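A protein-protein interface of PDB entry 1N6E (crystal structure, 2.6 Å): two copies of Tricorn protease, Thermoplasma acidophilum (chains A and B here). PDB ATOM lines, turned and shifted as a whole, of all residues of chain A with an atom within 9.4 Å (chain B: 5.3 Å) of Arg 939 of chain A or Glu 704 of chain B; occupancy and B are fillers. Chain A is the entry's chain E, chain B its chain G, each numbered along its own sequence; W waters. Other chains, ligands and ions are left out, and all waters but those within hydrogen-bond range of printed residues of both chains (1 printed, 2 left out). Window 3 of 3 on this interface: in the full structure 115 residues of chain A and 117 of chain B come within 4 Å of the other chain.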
ATOM      1  N   ASP A 936      21.377  21.772 -21.067  1.00  0.00           N
ATOM      2  CA  ASP A 936      21.526  20.352 -21.143  1.00  0.00           C
ATOM      3  C   ASP A 936      22.463  20.071 -22.301  1.00  0.00           C
ATOM      4  O   ASP A 936      22.213  20.537 -23.413  1.00  0.00           O
ATOM      5  CB  ASP A 936      20.146  19.750 -21.398  1.00  0.00           C
ATOM      6  CG  ASP A 936      20.150  18.248 -21.366  1.00  0.00           C
ATOM      7  OD1 ASP A 936      19.064  17.651 -21.506  1.00  0.00           O
ATOM      8  OD2 ASP A 936      21.241  17.676 -21.203  1.00  0.00           O
ATOM      9  N   ASN A 937      23.536  19.322 -22.041  1.00  0.00           N
ATOM     10  CA  ASN A 937      24.497  18.964 -23.072  1.00  0.00           C
ATOM     11  C   ASN A 937      24.405  17.536 -23.527  1.00  0.00           C
ATOM     12  O   ASN A 937      24.851  16.637 -22.817  1.00  0.00           O
ATOM     13  CB  ASN A 937      25.903  19.158 -22.582  1.00  0.00           C
ATOM     14  CG  ASN A 937      26.562  20.282 -23.242  1.00  0.00           C
ATOM     15  OD1 ASN A 937      26.283  21.415 -22.894  1.00  0.00           O
ATOM     16  ND2 ASN A 937      27.413  20.006 -24.234  1.00  0.00           N
ATOM     17  N   PRO A 938      23.906  17.312 -24.745  1.00  0.00           N
ATOM     18  CA  PRO A 938      23.763  15.964 -25.281  1.00  0.00           C
ATOM     19  C   PRO A 938      24.953  15.423 -26.047  1.00  0.00           C
ATOM     20  O   PRO A 938      25.784  16.173 -26.531  1.00  0.00           O
ATOM     21  CB  PRO A 938      22.563  16.111 -26.181  1.00  0.00           C
ATOM     22  CG  PRO A 938      22.890  17.445 -26.837  1.00  0.00           C
ATOM     23  CD  PRO A 938      23.345  18.304 -25.676  1.00  0.00           C
ATOM     24  N   ARG A 939      25.021  14.105 -26.168  1.00  0.00           N
ATOM     25  CA  ARG A 939      26.101  13.496 -26.926  1.00  0.00           C
ATOM     26  C   ARG A 939      25.896  13.908 -28.369  1.00  0.00           C
ATOM     27  O   ARG A 939      26.849  14.216 -29.072  1.00  0.00           O
ATOM     28  CB  ARG A 939      26.078  11.967 -26.829  1.00  0.00           C
ATOM     29  CG  ARG A 939      27.059  11.300 -27.783  1.00  0.00           C
ATOM     30  CD  ARG A 939      28.520  11.852 -27.649  1.00  0.00           C
ATOM     31  NE  ARG A 939      29.425  11.024 -28.445  1.00  0.00           N
ATOM     32  CZ  ARG A 939      29.764   9.760 -28.134  1.00  0.00           C
ATOM     33  NH1 ARG A 939      30.549   9.059 -28.942  1.00  0.00           N
ATOM     34  NH2 ARG A 939      29.361   9.210 -26.989  1.00  0.00           N
ATOM     35  N   ARG A 940      24.646  13.902 -28.816  1.00  0.00           N
ATOM     36  CA  ARG A 940      24.320  14.291 -30.187  1.00  0.00           C
ATOM     37  C   ARG A 940      23.126  15.239 -30.141  1.00  0.00           C
ATOM     38  O   ARG A 940      22.264  15.100 -29.280  1.00  0.00           O
ATOM     39  CB  ARG A 940      24.011  13.045 -31.037  1.00  0.00           C
ATOM     40  CG  ARG A 940      22.972  12.107 -30.466  1.00  0.00           C
ATOM     41  CD  ARG A 940      22.900  10.829 -31.314  1.00  0.00           C
ATOM     42  NE  ARG A 940      24.204  10.144 -31.360  1.00  0.00           N
ATOM     43  CZ  ARG A 940      24.651   9.349 -30.392  1.00  0.00           C
ATOM     44  NH1 ARG A 940      25.833   8.772 -30.502  1.00  0.00           N
ATOM     45  NH2 ARG A 940      23.888   9.120 -29.314  1.00  0.00           N
ATOM     46  N   GLY A 941      23.085  16.208 -31.045  1.00  0.00           N
ATOM     47  CA  GLY A 941      21.977  17.149 -31.051  1.00  0.00           C
ATOM     48  C   GLY A 941      22.396  18.505 -30.526  1.00  0.00           C
ATOM     49  O   GLY A 941      23.578  18.825 -30.488  1.00  0.00           O
ATOM     50  N   THR A 942      21.449  19.315 -30.094  1.00  0.00           N
ATOM     51  CA  THR A 942      21.805  20.639 -29.599  1.00  0.00           C
ATOM     52  C   THR A 942      21.446  20.829 -28.120  1.00  0.00           C
ATOM     53  O   THR A 942      20.809  19.965 -27.497  1.00  0.00           O
ATOM     54  CB  THR A 942      21.101  21.740 -30.453  1.00  0.00           C
ATOM     55  OG1 THR A 942      19.668  21.658 -30.284  1.00  0.00           O
ATOM     56  CG2 THR A 942      21.470  21.564 -31.954  1.00  0.00           C
ATOM     57  N   LEU A 943      21.852  21.967 -27.558  1.00  0.00           N
ATOM     58  CA  LEU A 943      21.568  22.281 -26.162  1.00  0.00           C
ATOM     59  C   LEU A 943      20.094  22.411 -25.854  1.00  0.00           C
ATOM     60  O   LEU A 943      19.333  22.921 -26.680  1.00  0.00           O
ATOM     61  CB  LEU A 943      22.179  23.615 -25.788  1.00  0.00           C
ATOM     62  CG  LEU A 943      23.663  23.784 -26.019  1.00  0.00           C
ATOM     63  CD1 LEU A 943      24.033  25.162 -25.554  1.00  0.00           C
ATOM     64  CD2 LEU A 943      24.436  22.739 -25.237  1.00  0.00           C
ATOM     65  N   ARG B 698      29.766   3.615 -24.699  1.00  0.00           N
ATOM     66  CA  ARG B 698      30.692   4.483 -25.421  1.00  0.00           C
ATOM     67  C   ARG B 698      30.014   5.463 -26.379  1.00  0.00           C
ATOM     68  O   ARG B 698      30.362   6.634 -26.413  1.00  0.00           O
ATOM     69  CB  ARG B 698      31.668   3.656 -26.225  1.00  0.00           C
ATOM     70  CG  ARG B 698      32.743   4.538 -26.811  1.00  0.00           C
ATOM     71  CD  ARG B 698      33.449   3.792 -27.906  1.00  0.00           C
ATOM     72  NE  ARG B 698      32.492   3.392 -28.928  1.00  0.00           N
ATOM     73  CZ  ARG B 698      32.803   2.722 -30.026  1.00  0.00           C
ATOM     74  NH1 ARG B 698      31.859   2.405 -30.925  1.00  0.00           N
ATOM     75  NH2 ARG B 698      34.058   2.369 -30.218  1.00  0.00           N
ATOM     76  N   ASP B 699      29.052   4.941 -27.145  1.00  0.00           N
ATOM     77  CA  ASP B 699      28.331   5.727 -28.114  1.00  0.00           C
ATOM     78  C   ASP B 699      27.437   6.827 -27.502  1.00  0.00           C
ATOM     79  O   ASP B 699      27.257   7.905 -28.104  1.00  0.00           O
ATOM     80  CB  ASP B 699      27.477   4.813 -29.002  1.00  0.00           C
ATOM     81  CG  ASP B 699      28.290   3.893 -29.900  1.00  0.00           C
ATOM     82  OD1 ASP B 699      27.670   2.963 -30.521  1.00  0.00           O
ATOM     83  OD2 ASP B 699      29.527   4.067 -30.007  1.00  0.00           O
ATOM     84  N   ASN B 700      26.878   6.566 -26.321  1.00  0.00           N
ATOM     85  CA  ASN B 700      25.987   7.529 -25.711  1.00  0.00           C
ATOM     86  C   ASN B 700      26.499   8.438 -24.599  1.00  0.00           C
ATOM     87  O   ASN B 700      25.814   9.413 -24.196  1.00  0.00           O
ATOM     88  CB  ASN B 700      24.714   6.842 -25.242  1.00  0.00           C
ATOM     89  CG  ASN B 700      23.999   6.141 -26.375  1.00  0.00           C
ATOM     90  OD1 ASN B 700      24.176   6.508 -27.550  1.00  0.00           O
ATOM     91  ND2 ASN B 700      23.200   5.136 -26.046  1.00  0.00           N
ATOM     92  N   TYR B 701      27.702   8.169 -24.113  1.00  0.00           N
ATOM     93  CA  TYR B 701      28.279   8.997 -23.059  1.00  0.00           C
ATOM     94  C   TYR B 701      28.257  10.428 -23.556  1.00  0.00           C
ATOM     95  O   TYR B 701      28.640  10.707 -24.689  1.00  0.00           O
ATOM     96  CB  TYR B 701      29.709   8.559 -22.763  1.00  0.00           C
ATOM     97  CG  TYR B 701      30.231   9.175 -21.503  1.00  0.00           C
ATOM     98  CD1 TYR B 701      29.622   8.916 -20.283  1.00  0.00           C
ATOM     99  CD2 TYR B 701      31.266  10.099 -21.543  1.00  0.00           C
ATOM    100  CE1 TYR B 701      30.006   9.563 -19.142  1.00  0.00           C
ATOM    101  CE2 TYR B 701      31.669  10.756 -20.405  1.00  0.00           C
ATOM    102  CZ  TYR B 701      31.026  10.490 -19.197  1.00  0.00           C
ATOM    103  OH  TYR B 701      31.351  11.206 -18.066  1.00  0.00           O
ATOM    104  N   TRP B 702      27.823  11.330 -22.696  1.00  0.00           N
ATOM    105  CA  TRP B 702      27.690  12.730 -23.063  1.00  0.00           C
ATOM    106  C   TRP B 702      28.957  13.378 -23.625  1.00  0.00           C
ATOM    107  O   TRP B 702      28.869  14.284 -24.453  1.00  0.00           O
ATOM    108  CB  TRP B 702      27.228  13.544 -21.864  1.00  0.00           C
ATOM    109  CG  TRP B 702      28.337  13.800 -20.878  1.00  0.00           C
ATOM    110  CD1 TRP B 702      28.837  12.927 -19.961  1.00  0.00           C
ATOM    111  CD2 TRP B 702      29.066  15.018 -20.712  1.00  0.00           C
ATOM    112  NE1 TRP B 702      29.814  13.523 -19.225  1.00  0.00           N
ATOM    113  CE2 TRP B 702      29.973  14.811 -19.653  1.00  0.00           C
ATOM    114  CE3 TRP B 702      29.022  16.283 -21.343  1.00  0.00           C
ATOM    115  CZ2 TRP B 702      30.851  15.808 -19.217  1.00  0.00           C
ATOM    116  CZ3 TRP B 702      29.890  17.274 -20.911  1.00  0.00           C
ATOM    117  CH2 TRP B 702      30.784  17.038 -19.849  1.00  0.00           C
ATOM    118  N   ASN B 703      30.126  12.934 -23.167  1.00  0.00           N
ATOM    119  CA  ASN B 703      31.378  13.488 -23.655  1.00  0.00           C
ATOM    120  C   ASN B 703      32.114  12.473 -24.549  1.00  0.00           C
ATOM    121  O   ASN B 703      32.615  11.440 -24.071  1.00  0.00           O
ATOM    122  CB  ASN B 703      32.245  13.890 -22.481  1.00  0.00           C
ATOM    123  CG  ASN B 703      33.533  14.564 -22.910  1.00  0.00           C
ATOM    124  OD1 ASN B 703      33.951  15.524 -22.288  1.00  0.00           O
ATOM    125  ND2 ASN B 703      34.178  14.057 -23.957  1.00  0.00           N
ATOM    126  N   GLU B 704      32.180  12.794 -25.847  1.00  0.00           N
ATOM    127  CA  GLU B 704      32.819  11.949 -26.845  1.00  0.00           C
ATOM    128  C   GLU B 704      34.305  11.710 -26.604  1.00  0.00           C
ATOM    129  O   GLU B 704      34.774  10.582 -26.689  1.00  0.00           O
ATOM    130  CB  GLU B 704      32.620  12.564 -28.219  1.00  0.00           C
ATOM    131  CG  GLU B 704      32.990  11.653 -29.375  1.00  0.00           C
ATOM    132  CD  GLU B 704      32.752  12.317 -30.718  1.00  0.00           C
ATOM    133  OE1 GLU B 704      32.886  11.622 -31.769  1.00  0.00           O
ATOM    134  OE2 GLU B 704      32.429  13.540 -30.711  1.00  0.00           O
ATOM    135  N   ALA B 705      35.058  12.762 -26.317  1.00  0.00           N
ATOM    136  CA  ALA B 705      36.482  12.571 -26.069  1.00  0.00           C
ATOM    137  C   ALA B 705      36.656  11.564 -24.929  1.00  0.00           C
ATOM    138  O   ALA B 705      37.339  10.541 -25.064  1.00  0.00           O
ATOM    139  CB  ALA B 705      37.145  13.889 -25.687  1.00  0.00           C
ATOM    140  N   VAL B 706      36.023  11.859 -23.801  1.00  0.00           N
ATOM    141  CA  VAL B 706      36.140  10.981 -22.667  1.00  0.00           C
ATOM    142  C   VAL B 706      35.747   9.559 -23.030  1.00  0.00           C
ATOM    143  O   VAL B 706      36.412   8.596 -22.639  1.00  0.00           O
ATOM    144  CB  VAL B 706      35.267  11.457 -21.519  1.00  0.00           C
ATOM    145  CG1 VAL B 706      35.296  10.436 -20.406  1.00  0.00           C
ATOM    146  CG2 VAL B 706      35.747  12.794 -21.040  1.00  0.00           C
ATOM    147  N   ALA B 707      34.668   9.429 -23.781  1.00  0.00           N
ATOM    148  CA  ALA B 707      34.212   8.118 -24.168  1.00  0.00           C
ATOM    149  C   ALA B 707      35.261   7.332 -24.942  1.00  0.00           C
ATOM    150  O   ALA B 707      35.313   6.111 -24.839  1.00  0.00           O
ATOM    151  CB  ALA B 707      32.906   8.231 -24.981  1.00  0.00           C
ATOM    152  N   LYS B 708      36.099   8.030 -25.709  1.00  0.00           N
ATOM    153  CA  LYS B 708      37.134   7.386 -26.524  1.00  0.00           C
ATOM    154  C   LYS B 708      38.189   6.724 -25.656  1.00  0.00           C
ATOM    155  O   LYS B 708      38.527   5.561 -25.863  1.00  0.00           O
ATOM    156  N   GLU B1010      24.015  10.533 -20.862  1.00  0.00           N
ATOM    157  CA  GLU B1010      24.097  11.186 -22.156  1.00  0.00           C
ATOM    158  C   GLU B1010      23.873  12.710 -22.199  1.00  0.00           C
ATOM    159  O   GLU B1010      24.295  13.382 -23.153  1.00  0.00           O
ATOM    160  CB  GLU B1010      23.093  10.494 -23.078  1.00  0.00           C
ATOM    161  CG  GLU B1010      23.007  10.969 -24.522  1.00  0.00           C
ATOM    162  CD  GLU B1010      22.423   9.879 -25.413  1.00  0.00           C
ATOM    163  OE1 GLU B1010      21.882   8.925 -24.832  1.00  0.00           O
ATOM    164  OE2 GLU B1010      22.486   9.946 -26.677  1.00  0.00           O
ATOM    165  N   PHE B1011      23.242  13.258 -21.167  1.00  0.00           N
ATOM    166  CA  PHE B1011      22.933  14.683 -21.146  1.00  0.00           C
ATOM    167  C   PHE B1011      23.441  15.428 -19.925  1.00  0.00           C
ATOM    168  O   PHE B1011      22.708  15.559 -18.948  1.00  0.00           O
ATOM    169  CB  PHE B1011      21.424  14.845 -21.207  1.00  0.00           C
ATOM    170  CG  PHE B1011      20.783  14.070 -22.304  1.00  0.00           C
ATOM    171  CD1 PHE B1011      20.486  12.738 -22.126  1.00  0.00           C
ATOM    172  CD2 PHE B1011      20.507  14.691 -23.539  1.00  0.00           C
ATOM    173  CE1 PHE B1011      19.943  12.015 -23.155  1.00  0.00           C
ATOM    174  CE2 PHE B1011      19.968  13.991 -24.580  1.00  0.00           C
ATOM    175  CZ  PHE B1011      19.674  12.640 -24.398  1.00  0.00           C
HETATM  176  O   HOH W   1      22.910  12.725 -27.288  1.00  0.00           O
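The backbone carbonyl oxygen (O) of Arg 698 of chain B is in hydrogen-bond range of the guanidinium group (NH2) of Arg 939 of chain A, at 2.8 Å.
The backbone carbonyl oxygen (O) of Asp 699 of chain B sits at hydrogen-bond distance from the guanidinium group (NH2) of Arg 939 of chain A (2.7 Å).
The guanidinium group of Arg 939 of chain A lies within hydrogen-bond range of the backbone carbonyl oxygen of Tyr 701 of chain B, at 2.8 Å.
The backbone NH (N) of Arg 939 of chain A sits at hydrogen-bond distance from the backbone carbonyl oxygen (O) of Glu 1010 of chain B, at 3.2 Å.
O of Asp 699 of chain B lies within hydrogen-bond range of NH1 of Arg 940 of chain A (2.9 Å).
NH2 of Arg 940 of chain A is in hydrogen-bond range of OD1 of Asn 700 of chain B.
OE2 of Glu 1010 of chain B is in salt-bridge range of NH2 of Arg 940 of chain A (3.1 Å).
The side-chain carboxylate (OD2) of Asp 936 of chain A lies close to the backbone carbonyl oxygen (O) of Phe 1011 of chain B, at 3.4 Å.
O of Asn 937 of chain A lies close to O of Glu 1010 of chain B (3.3 Å).
NH1 of Arg 698 of chain B lies within salt-bridge range of OD2 of Asp 699 of chain B (3.0 Å).
The indole nitrogen (NE1) of Trp 702 of chain B is in hydrogen-bond range of the side-chain hydroxyl (OH) of Tyr 701 of chain B (3.0 Å).
Among the printed residues, pairs that only touch across the chains: Asn 937 of chain A with Phe 1011 of chain B, Pro 938 of chain A with Glu 1010 of chain B, Pro 938 of chain A with Phe 1011 of chain B, Arg 939 of chain A with Asn 700 of chain B, Arg 939 of chain A with Trp 702 of chain B and Arg 939 of chain A with Glu 704 of chain B.
Of chain B, only Arg 698, Asp 699, Asn 700, Tyr 701, Trp 702, Glu 704 and Glu 1010 come within 4 Å of Arg 939 of chain A.
Of the printed residues of chain B, Arg 940 of chain A touches Asp 699, Asn 700 and Glu 1010.
Thr 942 of chain A touches none of the printed residues of chain B.
Printed residues of chain A within 4 Å of Asp 699 of chain B: Arg 939 (2.7 Å) and Arg 940 (2.9 Å).
Of the printed residues of chain A, Asn 700 of chain B touches Arg 939 (3.7 Å) and Arg 940 (3.2 Å).
Asn 703 of chain B touches none of the printed residues of chain A.
Printed residues of chain A within 4 Å of Glu 704 of chain B: Arg 939 (3.6 Å).
No residue of chain A comes within 4 Å of Ala 705 of chain B.
No residue of chain A comes within 4 Å of Ala 707 of chain B.
Printed residues of chain A within 4 Å of Glu 1010 of chain B: Asn 937, Pro 938, Arg 939 and Arg 940.
The nearest residue of chain B that does not touch Arg 939 of chain A is Ala 707 of chain B (4.2 Å).
Hydrophobic or aromatic side chains of chain A that line the printed part of chain B: Pro 938.
Of the 13 printed residues of chain B, 8 touch a printed residue of chain A.
Hydrophobic or aromatic side chains of chain B within 4 Å of the printed part of chain A: Phe 1011.
No position is printed for both chains.
Of the 15 pairs that touch across the chains among the printed residues, none has its exchanged pair printed and touching as well.
Water W1 lies within hydrogen-bond range of N of Arg 940 of chain A (2.6 Å), N of Arg 939 of chain A (2.8 Å) and OE2 of Glu 1010 of chain B (2.9 Å).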
